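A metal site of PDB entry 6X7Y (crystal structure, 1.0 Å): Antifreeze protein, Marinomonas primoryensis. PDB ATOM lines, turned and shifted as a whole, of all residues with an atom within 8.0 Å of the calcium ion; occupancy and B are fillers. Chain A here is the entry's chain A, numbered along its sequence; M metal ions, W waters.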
ATOM      1  N   TYR A  12      -9.345  23.646  17.892  1.00  0.00           N
ATOM      2  CA  TYR A  12      -8.272  24.561  18.311  1.00  0.00           C
ATOM      3  C   TYR A  12      -8.861  25.907  18.673  1.00  0.00           C
ATOM      4  O   TYR A  12      -9.721  26.423  17.938  1.00  0.00           O
ATOM      5  CB  TYR A  12      -7.246  24.720  17.175  1.00  0.00           C
ATOM      6  CG  TYR A  12      -6.288  25.853  17.440  1.00  0.00           C
ATOM      7  CD1 TYR A  12      -5.226  25.691  18.319  1.00  0.00           C
ATOM      8  CD2 TYR A  12      -6.478  27.097  16.886  1.00  0.00           C
ATOM      9  CE1 TYR A  12      -4.378  26.740  18.642  1.00  0.00           C
ATOM     10  CE2 TYR A  12      -5.645  28.157  17.186  1.00  0.00           C
ATOM     11  CZ  TYR A  12      -4.585  27.987  18.070  1.00  0.00           C
ATOM     12  OH  TYR A  12      -3.760  29.023  18.403  1.00  0.00           O
ATOM     13  N   VAL A  52       2.714  28.115  19.999  1.00  0.00           N
ATOM     14  CA  VAL A  52       1.894  27.274  19.115  1.00  0.00           C
ATOM     15  C   VAL A  52       0.930  28.115  18.283  1.00  0.00           C
ATOM     16  O   VAL A  52       0.546  27.707  17.190  1.00  0.00           O
ATOM     17  CB  VAL A  52       1.132  26.179  19.880  1.00  0.00           C
ATOM     18  CG1 VAL A  52      -0.157  26.660  20.499  1.00  0.00           C
ATOM     19  CG2 VAL A  52       0.857  24.981  18.957  1.00  0.00           C
ATOM     20  N   ALA A  53       0.509  29.256  18.846  1.00  0.00           N
ATOM     21  CA  ALA A  53      -0.578  30.029  18.266  1.00  0.00           C
ATOM     22  C   ALA A  53      -0.107  31.023  17.191  1.00  0.00           C
ATOM     23  O   ALA A  53      -0.947  31.734  16.622  1.00  0.00           O
ATOM     24  CB  ALA A  53      -1.353  30.731  19.378  1.00  0.00           C
ATOM     25  N   LYS A  54       1.207  31.051  16.935  1.00  0.00           N
ATOM     26  CA  LYS A  54       1.760  31.987  15.942  1.00  0.00           C
ATOM     27  C   LYS A  54       2.096  31.299  14.618  1.00  0.00           C
ATOM     28  O   LYS A  54       2.473  30.108  14.613  1.00  0.00           O
ATOM     29  CB  LYS A  54       3.009  32.665  16.509  1.00  0.00           C
ATOM     30  CG  LYS A  54       2.651  33.518  17.707  1.00  0.00           C
ATOM     31  CD  LYS A  54       3.195  34.867  17.842  1.00  0.00           C
ATOM     32  CE  LYS A  54       2.353  35.714  18.775  1.00  0.00           C
ATOM     33  NZ  LYS A  54       3.190  36.865  19.157  1.00  0.00           N
ATOM     34  N   GLY A  55       1.913  32.030  13.525  1.00  0.00           N
ATOM     35  CA  GLY A  55       2.366  31.552  12.222  1.00  0.00           C
ATOM     36  C   GLY A  55       1.808  30.198  11.881  1.00  0.00           C
ATOM     37  O   GLY A  55       0.613  29.944  12.036  1.00  0.00           O
ATOM     38  N   THR A  56       2.698  29.333  11.410  1.00  0.00           N
ATOM     39  CA  THR A  56       2.321  27.956  11.015  1.00  0.00           C
ATOM     40  C   THR A  56       2.705  26.934  12.082  1.00  0.00           C
ATOM     41  O   THR A  56       2.802  25.729  11.814  1.00  0.00           O
ATOM     42  CB  THR A  56       2.956  27.597   9.670  1.00  0.00           C
ATOM     43  OG1 THR A  56       4.379  27.667   9.742  1.00  0.00           O
ATOM     44  CG2 THR A  56       2.496  28.508   8.571  1.00  0.00           C
ATOM     45  N   HIS A  57       2.917  27.405  13.315  1.00  0.00           N
ATOM     46  CA  HIS A  57       3.343  26.480  14.371  1.00  0.00           C
ATOM     47  C   HIS A  57       2.298  25.434  14.690  1.00  0.00           C
ATOM     48  O   HIS A  57       2.641  24.302  15.024  1.00  0.00           O
ATOM     49  CB  HIS A  57       3.758  27.271  15.607  1.00  0.00           C
ATOM     50  CG  HIS A  57       4.941  28.138  15.334  1.00  0.00           C
ATOM     51  ND1 HIS A  57       5.230  29.261  16.086  1.00  0.00           N
ATOM     52  CD2 HIS A  57       5.910  28.080  14.398  1.00  0.00           C
ATOM     53  CE1 HIS A  57       6.305  29.854  15.586  1.00  0.00           C
ATOM     54  NE2 HIS A  57       6.747  29.153  14.570  1.00  0.00           N
ATOM     55  N   LEU A  58       0.997  25.783  14.622  1.00  0.00           N
ATOM     56  CA  LEU A  58      -0.033  24.791  14.884  1.00  0.00           C
ATOM     57  C   LEU A  58       0.027  23.647  13.884  1.00  0.00           C
ATOM     58  O   LEU A  58      -0.105  22.478  14.226  1.00  0.00           O
ATOM     59  CB  LEU A  58      -1.408  25.445  14.881  1.00  0.00           C
ATOM     60  CG  LEU A  58      -2.579  24.484  15.091  1.00  0.00           C
ATOM     61  CD1 LEU A  58      -2.578  23.865  16.463  1.00  0.00           C
ATOM     62  CD2 LEU A  58      -3.900  25.193  14.815  1.00  0.00           C
ATOM     63  N   GLN A  59       0.200  24.015  12.607  1.00  0.00           N
ATOM     64  CA  GLN A  59       0.306  23.037  11.552  1.00  0.00           C
ATOM     65  C   GLN A  59       1.471  22.077  11.826  1.00  0.00           C
ATOM     66  O   GLN A  59       1.367  20.863  11.649  1.00  0.00           O
ATOM     67  CB  GLN A  59       0.544  23.709  10.186  1.00  0.00           C
ATOM     68  CG  GLN A  59      -0.659  24.394   9.576  1.00  0.00           C
ATOM     69  CD  GLN A  59      -1.051  25.746  10.150  1.00  0.00           C
ATOM     70  OE1 GLN A  59      -0.475  26.285  11.090  1.00  0.00           O
ATOM     71  NE2 GLN A  59      -2.076  26.334   9.521  1.00  0.00           N
ATOM     72  N   LEU A  69      -7.178  20.323   8.933  1.00  0.00           N
ATOM     73  CA  LEU A  69      -7.583  21.593   9.482  1.00  0.00           C
ATOM     74  C   LEU A  69      -8.649  22.254   8.607  1.00  0.00           C
ATOM     75  O   LEU A  69      -8.544  22.343   7.385  1.00  0.00           O
ATOM     76  CB  LEU A  69      -6.386  22.554   9.574  1.00  0.00           C
ATOM     77  CG  LEU A  69      -5.517  22.346  10.824  1.00  0.00           C
ATOM     78  CD1 LEU A  69      -4.149  23.021  10.611  1.00  0.00           C
ATOM     79  CD2 LEU A  69      -6.186  22.877  12.049  1.00  0.00           C
ATOM     80  N   THR A  71      -9.325  25.484   8.690  1.00  0.00           N
ATOM     81  CA  THR A  71      -8.823  26.788   8.350  1.00  0.00           C
ATOM     82  C   THR A  71      -7.436  26.912   8.934  1.00  0.00           C
ATOM     83  O   THR A  71      -7.032  26.112   9.780  1.00  0.00           O
ATOM     84  CB  THR A  71      -9.806  27.860   8.823  1.00  0.00           C
ATOM     85  OG1 THR A  71      -9.507  29.108   8.223  1.00  0.00           O
ATOM     86  CG2 THR A  71      -9.821  27.942  10.316  1.00  0.00           C
ATOM     87  N   ASP A  72      -6.708  27.959   8.505  1.00  0.00           N
ATOM     88  CA  ASP A  72      -5.441  28.334   9.090  1.00  0.00           C
ATOM     89  C   ASP A  72      -5.706  29.492  10.045  1.00  0.00           C
ATOM     90  O   ASP A  72      -5.966  30.610   9.588  1.00  0.00           O
ATOM     91  CB  ASP A  72      -4.467  28.792   8.001  1.00  0.00           C
ATOM     92  CG  ASP A  72      -3.124  29.290   8.518  1.00  0.00           C
ATOM     93  OD1 ASP A  72      -2.897  29.188   9.758  1.00  0.00           O
ATOM     94  OD2 ASP A  72      -2.328  29.742   7.677  1.00  0.00           O
ATOM     95  N   PRO A  73      -5.719  29.285  11.374  1.00  0.00           N
ATOM     96  CA  PRO A  73      -5.984  30.375  12.294  1.00  0.00           C
ATOM     97  C   PRO A  73      -4.986  31.523  12.120  1.00  0.00           C
ATOM     98  O   PRO A  73      -3.828  31.318  11.755  1.00  0.00           O
ATOM     99  CB  PRO A  73      -5.845  29.729  13.676  1.00  0.00           C
ATOM    100  CG  PRO A  73      -5.763  28.303  13.485  1.00  0.00           C
ATOM    101  CD  PRO A  73      -5.372  28.021  12.065  1.00  0.00           C
ATOM    102  N   GLY A  74      -5.445  32.738  12.423  1.00  0.00           N
ATOM    103  CA  GLY A  74      -4.535  33.853  12.554  1.00  0.00           C
ATOM    104  C   GLY A  74      -3.690  33.751  13.817  1.00  0.00           C
ATOM    105  O   GLY A  74      -3.801  32.796  14.610  1.00  0.00           O
ATOM    106  N   ASP A  75      -2.812  34.748  14.004  1.00  0.00           N
ATOM    107  CA  ASP A  75      -1.940  34.721  15.156  1.00  0.00           C
ATOM    108  C   ASP A  75      -2.716  34.990  16.444  1.00  0.00           C
ATOM    109  O   ASP A  75      -3.595  35.856  16.512  1.00  0.00           O
ATOM    110  CB  ASP A  75      -0.849  35.778  15.042  1.00  0.00           C
ATOM    111  CG  ASP A  75       0.283  35.467  14.084  1.00  0.00           C
ATOM    112  OD1 ASP A  75       0.313  34.366  13.502  1.00  0.00           O
ATOM    113  OD2 ASP A  75       1.126  36.378  13.909  1.00  0.00           O
ATOM    114  N   ASN A  76      -2.268  34.299  17.504  1.00  0.00           N
ATOM    115  CA  ASN A  76      -2.631  34.618  18.896  1.00  0.00           C
ATOM    116  C   ASN A  76      -1.372  34.397  19.727  1.00  0.00           C
ATOM    117  O   ASN A  76      -0.419  33.782  19.263  1.00  0.00           O
ATOM    118  CB  ASN A  76      -3.817  33.720  19.455  1.00  0.00           C
ATOM    119  CG  ASN A  76      -5.165  34.169  18.962  1.00  0.00           C
ATOM    120  OD1 ASN A  76      -5.617  35.262  19.391  1.00  0.00           O
ATOM    121  ND2 ASN A  76      -5.795  33.387  18.192  1.00  0.00           N
HETATM  122 CA    CA M   1      -1.657  30.495  11.444  1.00  0.00          CA
HETATM  123  O   HOH W   1      -0.531  30.825   9.382  1.00  0.00           O
HETATM  124  O   HOH W   2      -1.013  32.826  11.597  1.00  0.00           O
HETATM  125  O   HOH W   3      -1.840  30.914  13.826  1.00  0.00           O
HETATM  126  O   HOH W   4      -1.804  28.292  12.459  1.00  0.00           O
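OD1 of Asp 75 sits at hydrogen-bond distance from N of Gly 55, at 2.8 Å. OD1 of Asp 72 lies close to NE2 of Gln 59 (3.0 Å).
Three residues have an atom within 4 Å of the calcium ion: Gly 55, Asp 72 and Pro 73.
The calcium ion is bound by O of Pro 73 (2.3 Å). Water W1 binds the calcium ion (2.4 Å). The backbone carbonyl oxygen (O) of Gly 55 binds the calcium ion (2.4 Å). Water W2 is bound to the calcium ion, at 2.4 Å. Water W3 is bound to the calcium ion, 2.4 Å away. Water W4 is bound to the calcium ion (2.4 Å). OD1 of Asp 72 binds the calcium ion (2.5 Å).
Water W3 lies within hydrogen-bond range of the backbone carbonyl oxygen (O) of Gly 74 (2.8 Å) and the backbone carbonyl oxygen (O) of Ala 53 (3.0 Å).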
